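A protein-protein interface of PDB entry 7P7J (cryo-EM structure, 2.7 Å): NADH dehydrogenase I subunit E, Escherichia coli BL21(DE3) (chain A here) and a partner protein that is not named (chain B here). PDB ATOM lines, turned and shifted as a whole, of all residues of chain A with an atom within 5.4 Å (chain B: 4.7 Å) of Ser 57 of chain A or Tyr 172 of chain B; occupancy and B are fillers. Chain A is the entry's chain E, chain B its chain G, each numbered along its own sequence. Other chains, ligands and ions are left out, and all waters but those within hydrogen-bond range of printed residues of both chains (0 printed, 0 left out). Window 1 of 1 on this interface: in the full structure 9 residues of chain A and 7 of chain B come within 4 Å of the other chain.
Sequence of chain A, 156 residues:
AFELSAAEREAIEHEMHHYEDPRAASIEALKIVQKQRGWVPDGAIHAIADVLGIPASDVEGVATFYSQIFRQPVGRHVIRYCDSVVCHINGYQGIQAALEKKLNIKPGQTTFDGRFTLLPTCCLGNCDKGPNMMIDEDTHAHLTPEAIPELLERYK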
ATOM      1  N   PRO A  55     -33.160  23.491   5.314  1.00  0.00           N
ATOM      2  CA  PRO A  55     -32.803  24.670   6.112  1.00  0.00           C
ATOM      3  C   PRO A  55     -31.309  24.955   6.106  1.00  0.00           C
ATOM      4  O   PRO A  55     -30.480  24.054   5.967  1.00  0.00           O
ATOM      5  CB  PRO A  55     -33.287  24.305   7.519  1.00  0.00           C
ATOM      6  CG  PRO A  55     -34.345  23.308   7.305  1.00  0.00           C
ATOM      7  CD  PRO A  55     -33.923  22.515   6.113  1.00  0.00           C
ATOM      8  N   ALA A  56     -30.976  26.239   6.261  1.00  0.00           N
ATOM      9  CA  ALA A  56     -29.580  26.661   6.266  1.00  0.00           C
ATOM     10  C   ALA A  56     -28.830  26.143   7.484  1.00  0.00           C
ATOM     11  O   ALA A  56     -27.603  26.013   7.439  1.00  0.00           O
ATOM     12  CB  ALA A  56     -29.490  28.184   6.201  1.00  0.00           C
ATOM     13  N   SER A  57     -29.541  25.855   8.578  1.00  0.00           N
ATOM     14  CA  SER A  57     -28.894  25.264   9.744  1.00  0.00           C
ATOM     15  C   SER A  57     -28.376  23.866   9.436  1.00  0.00           C
ATOM     16  O   SER A  57     -27.303  23.482   9.911  1.00  0.00           O
ATOM     17  CB  SER A  57     -29.858  25.235  10.928  1.00  0.00           C
ATOM     18  OG  SER A  57     -31.051  24.549  10.604  1.00  0.00           O
ATOM     19  N   ASP A  58     -29.117  23.097   8.633  1.00  0.00           N
ATOM     20  CA  ASP A  58     -28.656  21.771   8.230  1.00  0.00           C
ATOM     21  C   ASP A  58     -27.407  21.849   7.360  1.00  0.00           C
ATOM     22  O   ASP A  58     -26.460  21.076   7.555  1.00  0.00           O
ATOM     23  CB  ASP A  58     -29.772  21.034   7.493  1.00  0.00           C
ATOM     24  CG  ASP A  58     -30.911  20.640   8.406  1.00  0.00           C
ATOM     25  OD1 ASP A  58     -31.851  19.970   7.932  1.00  0.00           O
ATOM     26  OD2 ASP A  58     -30.867  20.999   9.600  1.00  0.00           O
ATOM     27  N   VAL A  59     -27.382  22.784   6.406  1.00  0.00           N
ATOM     28  CA  VAL A  59     -26.216  22.942   5.543  1.00  0.00           C
ATOM     29  C   VAL A  59     -25.019  23.432   6.346  1.00  0.00           C
ATOM     30  O   VAL A  59     -23.883  23.004   6.112  1.00  0.00           O
ATOM     31  CB  VAL A  59     -26.542  23.885   4.372  1.00  0.00           C
ATOM     32  CG1 VAL A  59     -25.406  23.907   3.367  1.00  0.00           C
ATOM     33  CG2 VAL A  59     -27.827  23.463   3.698  1.00  0.00           C
ATOM     34  N   GLU A  60     -25.252  24.328   7.308  1.00  0.00           N
ATOM     35  CA  GLU A  60     -24.167  24.801   8.161  1.00  0.00           C
ATOM     36  C   GLU A  60     -23.628  23.685   9.045  1.00  0.00           C
ATOM     37  O   GLU A  60     -22.413  23.583   9.247  1.00  0.00           O
ATOM     38  CB  GLU A  60     -24.646  25.978   9.010  1.00  0.00           C
ATOM     39  CG  GLU A  60     -23.576  26.573   9.907  1.00  0.00           C
ATOM     40  CD  GLU A  60     -22.548  27.375   9.139  1.00  0.00           C
ATOM     41  OE1 GLU A  60     -22.881  27.876   8.047  1.00  0.00           O
ATOM     42  OE2 GLU A  60     -21.407  27.509   9.627  1.00  0.00           O
ATOM     43  N   GLY A  61     -24.512  22.835   9.573  1.00  0.00           N
ATOM     44  CA  GLY A  61     -24.060  21.711  10.372  1.00  0.00           C
ATOM     45  C   GLY A  61     -23.269  20.701   9.566  1.00  0.00           C
ATOM     46  O   GLY A  61     -22.286  20.138  10.054  1.00  0.00           O
ATOM     47  N   VAL A  62     -23.676  20.469   8.317  1.00  0.00           N
ATOM     48  CA  VAL A  62     -22.908  19.591   7.441  1.00  0.00           C
ATOM     49  C   VAL A  62     -21.550  20.206   7.117  1.00  0.00           C
ATOM     50  O   VAL A  62     -20.519  19.530   7.186  1.00  0.00           O
ATOM     51  CB  VAL A  62     -23.716  19.267   6.172  1.00  0.00           C
ATOM     52  CG1 VAL A  62     -22.845  18.606   5.128  1.00  0.00           C
ATOM     53  CG2 VAL A  62     -24.879  18.362   6.517  1.00  0.00           C
ATOM     54  N   THR A  64     -19.786  22.457   8.792  1.00  0.00           N
ATOM     55  CA  THR A  64     -18.920  22.493   9.960  1.00  0.00           C
ATOM     56  C   THR A  64     -18.581  21.108  10.488  1.00  0.00           C
ATOM     57  O   THR A  64     -17.606  20.969  11.234  1.00  0.00           O
ATOM     58  CB  THR A  64     -19.574  23.308  11.073  1.00  0.00           C
ATOM     59  OG1 THR A  64     -20.909  22.838  11.273  1.00  0.00           O
ATOM     60  CG2 THR A  64     -19.611  24.778  10.706  1.00  0.00           C
ATOM     61  N   LYS B 161     -36.386  21.329  16.052  1.00  0.00           N
ATOM     62  CA  LYS B 161     -36.478  20.878  14.674  1.00  0.00           C
ATOM     63  C   LYS B 161     -37.498  19.756  14.511  1.00  0.00           C
ATOM     64  O   LYS B 161     -38.449  19.893  13.737  1.00  0.00           O
ATOM     65  CB  LYS B 161     -35.092  20.431  14.194  1.00  0.00           C
ATOM     66  CG  LYS B 161     -34.981  20.184  12.706  1.00  0.00           C
ATOM     67  CD  LYS B 161     -33.528  20.048  12.293  1.00  0.00           C
ATOM     68  CE  LYS B 161     -32.730  21.283  12.679  1.00  0.00           C
ATOM     69  NZ  LYS B 161     -31.287  21.146  12.352  1.00  0.00           N
ATOM     70  N   THR B 167     -36.541  25.900  11.871  1.00  0.00           N
ATOM     71  CA  THR B 167     -35.476  25.651  10.915  1.00  0.00           C
ATOM     72  C   THR B 167     -34.150  26.307  11.264  1.00  0.00           C
ATOM     73  O   THR B 167     -33.114  25.838  10.784  1.00  0.00           O
ATOM     74  CB  THR B 167     -35.889  26.124   9.512  1.00  0.00           C
ATOM     75  OG1 THR B 167     -36.060  27.546   9.517  1.00  0.00           O
ATOM     76  CG2 THR B 167     -37.189  25.468   9.084  1.00  0.00           C
ATOM     77  N   ASP B 168     -34.144  27.362  12.074  1.00  0.00           N
ATOM     78  CA  ASP B 168     -32.947  28.172  12.235  1.00  0.00           C
ATOM     79  C   ASP B 168     -32.038  27.726  13.374  1.00  0.00           C
ATOM     80  O   ASP B 168     -30.934  28.261  13.496  1.00  0.00           O
ATOM     81  CB  ASP B 168     -33.328  29.640  12.439  1.00  0.00           C
ATOM     82  CG  ASP B 168     -34.447  29.818  13.433  1.00  0.00           C
ATOM     83  OD1 ASP B 168     -35.370  28.982  13.447  1.00  0.00           O
ATOM     84  OD2 ASP B 168     -34.408  30.799  14.198  1.00  0.00           O
ATOM     85  N   LEU B 169     -32.448  26.772  14.200  1.00  0.00           N
ATOM     86  CA  LEU B 169     -31.578  26.245  15.243  1.00  0.00           C
ATOM     87  C   LEU B 169     -31.021  24.896  14.818  1.00  0.00           C
ATOM     88  O   LEU B 169     -31.725  24.085  14.210  1.00  0.00           O
ATOM     89  CB  LEU B 169     -32.317  26.104  16.573  1.00  0.00           C
ATOM     90  CG  LEU B 169     -31.467  25.909  17.828  1.00  0.00           C
ATOM     91  CD1 LEU B 169     -31.151  27.240  18.465  1.00  0.00           C
ATOM     92  CD2 LEU B 169     -32.171  25.004  18.815  1.00  0.00           C
ATOM     93  N   GLY B 170     -29.754  24.662  15.136  1.00  0.00           N
ATOM     94  CA  GLY B 170     -29.113  23.435  14.722  1.00  0.00           C
ATOM     95  C   GLY B 170     -27.832  23.191  15.486  1.00  0.00           C
ATOM     96  O   GLY B 170     -27.402  23.999  16.314  1.00  0.00           O
ATOM     97  N   VAL B 171     -27.233  22.043  15.188  1.00  0.00           N
ATOM     98  CA  VAL B 171     -25.978  21.609  15.785  1.00  0.00           C
ATOM     99  C   VAL B 171     -24.894  21.686  14.719  1.00  0.00           C
ATOM    100  O   VAL B 171     -25.073  21.203  13.596  1.00  0.00           O
ATOM    101  CB  VAL B 171     -26.103  20.197  16.391  1.00  0.00           C
ATOM    102  CG1 VAL B 171     -26.792  19.242  15.432  1.00  0.00           C
ATOM    103  CG2 VAL B 171     -24.743  19.657  16.807  1.00  0.00           C
ATOM    104  N   TYR B 172     -23.792  22.337  15.060  1.00  0.00           N
ATOM    105  CA  TYR B 172     -22.653  22.532  14.185  1.00  0.00           C
ATOM    106  C   TYR B 172     -21.405  21.988  14.855  1.00  0.00           C
ATOM    107  O   TYR B 172     -21.398  21.654  16.040  1.00  0.00           O
ATOM    108  CB  TYR B 172     -22.475  24.015  13.844  1.00  0.00           C
ATOM    109  CG  TYR B 172     -23.792  24.717  13.727  1.00  0.00           C
ATOM    110  CD1 TYR B 172     -24.626  24.480  12.647  1.00  0.00           C
ATOM    111  CD2 TYR B 172     -24.226  25.580  14.717  1.00  0.00           C
ATOM    112  CE1 TYR B 172     -25.839  25.103  12.542  1.00  0.00           C
ATOM    113  CE2 TYR B 172     -25.438  26.207  14.619  1.00  0.00           C
ATOM    114  CZ  TYR B 172     -26.241  25.964  13.530  1.00  0.00           C
ATOM    115  OH  TYR B 172     -27.458  26.585  13.432  1.00  0.00           O
ATOM    116  N   GLY B 173     -20.346  21.890  14.077  1.00  0.00           N
ATOM    117  CA  GLY B 173     -19.090  21.459  14.626  1.00  0.00           C
ATOM    118  C   GLY B 173     -18.974  19.950  14.710  1.00  0.00           C
ATOM    119  O   GLY B 173     -19.642  19.189  14.009  1.00  0.00           O
ATOM    120  N   ALA B 174     -18.112  19.525  15.625  1.00  0.00           N
ATOM    121  CA  ALA B 174     -17.575  18.174  15.618  1.00  0.00           C
ATOM    122  C   ALA B 174     -17.255  17.708  17.028  1.00  0.00           C
ATOM    123  O   ALA B 174     -17.793  18.233  18.005  1.00  0.00           O
ATOM    124  CB  ALA B 174     -16.334  18.093  14.731  1.00  0.00           C
ATOM    125  N   ASN B 177     -16.346  20.004  20.041  1.00  0.00           N
ATOM    126  CA  ASN B 177     -16.671  21.394  19.778  1.00  0.00           C
ATOM    127  C   ASN B 177     -18.068  21.537  19.183  1.00  0.00           C
ATOM    128  O   ASN B 177     -18.295  22.396  18.332  1.00  0.00           O
ATOM    129  CB  ASN B 177     -15.631  22.010  18.847  1.00  0.00           C
ATOM    130  CG  ASN B 177     -15.182  23.376  19.303  1.00  0.00           C
ATOM    131  OD1 ASN B 177     -14.956  23.602  20.490  1.00  0.00           O
ATOM    132  ND2 ASN B 177     -15.055  24.300  18.361  1.00  0.00           N
ATOM    133  N   VAL B 178     -19.005  20.687  19.607  1.00  0.00           N
ATOM    134  CA  VAL B 178     -20.374  20.780  19.118  1.00  0.00           C
ATOM    135  C   VAL B 178     -21.011  22.070  19.609  1.00  0.00           C
ATOM    136  O   VAL B 178     -20.978  22.391  20.804  1.00  0.00           O
ATOM    137  CB  VAL B 178     -21.195  19.553  19.543  1.00  0.00           C
ATOM    138  CG1 VAL B 178     -20.939  18.394  18.614  1.00  0.00           C
ATOM    139  CG2 VAL B 178     -20.849  19.150  20.964  1.00  0.00           C
ATOM    140  N   TYR B 179     -21.584  22.822  18.680  1.00  0.00           N
ATOM    141  CA  TYR B 179     -22.225  24.096  18.952  1.00  0.00           C
ATOM    142  C   TYR B 179     -23.710  23.967  18.672  1.00  0.00           C
ATOM    143  O   TYR B 179     -24.110  23.322  17.705  1.00  0.00           O
ATOM    144  CB  TYR B 179     -21.616  25.197  18.091  1.00  0.00           C
ATOM    145  CG  TYR B 179     -21.766  26.589  18.641  1.00  0.00           C
ATOM    146  CD1 TYR B 179     -22.916  27.326  18.403  1.00  0.00           C
ATOM    147  CD2 TYR B 179     -20.756  27.172  19.387  1.00  0.00           C
ATOM    148  CE1 TYR B 179     -23.057  28.600  18.896  1.00  0.00           C
ATOM    149  CE2 TYR B 179     -20.887  28.450  19.882  1.00  0.00           C
ATOM    150  CZ  TYR B 179     -22.040  29.157  19.637  1.00  0.00           C
ATOM    151  OH  TYR B 179     -22.176  30.430  20.133  1.00  0.00           O
ATOM    152  N   GLY B 181     -27.030  26.309  18.135  1.00  0.00           N
ATOM    153  CA  GLY B 181     -27.518  27.665  17.970  1.00  0.00           C
ATOM    154  C   GLY B 181     -27.930  27.926  16.539  1.00  0.00           C
ATOM    155  O   GLY B 181     -28.222  27.001  15.784  1.00  0.00           O
ATOM    156  N   ARG B 182     -27.969  29.183  16.195  1.00  0.00           N
ATOM    157  CA  ARG B 182     -28.263  29.610  14.841  1.00  0.00           C
ATOM    158  C   ARG B 182     -26.973  29.735  14.044  1.00  0.00           C
ATOM    159  O   ARG B 182     -25.896  29.895  14.625  1.00  0.00           O
ATOM    160  CB  ARG B 182     -29.012  30.938  14.872  1.00  0.00           C
ATOM    161  CG  ARG B 182     -30.337  30.878  15.595  1.00  0.00           C
ATOM    162  CD  ARG B 182     -31.078  32.194  15.496  1.00  0.00           C
ATOM    163  NE  ARG B 182     -31.745  32.358  14.211  1.00  0.00           N
ATOM    164  CZ  ARG B 182     -31.289  33.113  13.223  1.00  0.00           C
ATOM    165  NH1 ARG B 182     -30.156  33.785  13.334  1.00  0.00           N
ATOM    166  NH2 ARG B 182     -31.986  33.196  12.095  1.00  0.00           N
ATOM    167  N   PRO B 183     -27.032  29.627  12.710  1.00  0.00           N
ATOM    168  CA  PRO B 183     -25.803  29.817  11.919  1.00  0.00           C
ATOM    169  C   PRO B 183     -25.221  31.215  12.027  1.00  0.00           C
ATOM    170  O   PRO B 183     -24.007  31.388  11.863  1.00  0.00           O
ATOM    171  CB  PRO B 183     -26.253  29.496  10.488  1.00  0.00           C
ATOM    172  CG  PRO B 183     -27.717  29.684  10.495  1.00  0.00           C
ATOM    173  CD  PRO B 183     -28.176  29.273  11.850  1.00  0.00           C
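Ser 57 of chain A touches four residues of chain B. Of chain A, only Ser 57, Glu 60, Gly 61 and Thr 64 come within 4 Å of Tyr 172 of chain B. Of the printed residues of chain B, Thr 64 of chain A touches Tyr 172 (3.2 Å) and Gly 173 (3.0 Å). Printed residues of chain A within 4 Å of Thr 167 of chain B: Pro 55 and Ser 57. Ala 56 of chain A touches none of the printed residues of chain B.
The side-chain hydroxyl of Thr 64 of chain A sits at hydrogen-bond distance from the backbone carbonyl oxygen of Glu 60 of chain A, at 2.6 Å. The backbone NH (N) of Gly 170 of chain B is in hydrogen-bond range of the side-chain hydroxyl (OH) of Tyr 172 of chain B, 3.4 Å away. O of Gly 61 of chain A is in hydrogen-bond range of OG1 of Thr 64 of chain A (3.3 Å). The backbone carbonyl oxygen of Gly 181 of chain B is in hydrogen-bond range of the side-chain hydroxyl of Tyr 172 of chain B. The backbone NH (N) of Tyr 172 of chain B sits at hydrogen-bond distance from the backbone carbonyl oxygen (O) of Tyr 179 of chain B (2.8 Å).
Thr 167 of chain B touches Pro 55 of chain A. Ser 57 of chain A touches Lys 161 of chain B (OG to NZ, 3.8 Å). OG of Ser 57 of chain A touches O of Leu 169 of chain B (3.7 Å). Tyr 172 of chain B touches Ser 57 of chain A (CE1 to O, 3.4 Å). CG of Glu 60 of chain A touches CD1 of Tyr 172 of chain B, 3.6 Å away. O of Val 171 of chain B touches CA of Gly 61 of chain A (3.4 Å). Tyr 172 of chain B touches Gly 61 of chain A. Thr 64 of chain A touches Tyr 172 of chain B.
The side-chain hydroxyl (OG1) of Thr 64 of chain A sits at hydrogen-bond distance from the backbone NH (N) of Gly 173 of chain B (3.0 Å). O of Thr 167 of chain B lies within hydrogen-bond range of OG of Ser 57 of chain A (2.4 Å). The side-chain amino group (NZ) of Lys 161 of chain B is in salt-bridge range of the side-chain carboxylate (OD2) of Asp 58 of chain A, at 2.8 Å.
Of the 9 printed residues of chain A, 6 touch a printed residue of chain B. Of the 15 printed residues of chain B, 6 touch a printed residue of chain A. Among the printed residues, 11 pairs touch across the chains. Among the printed residues, Asp or Glu carboxylates within 4 Å of a Lys or Arg side-chain nitrogen of the other chain: Asp 58 of chain A with Lys 161 of chain B (2.8 Å).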
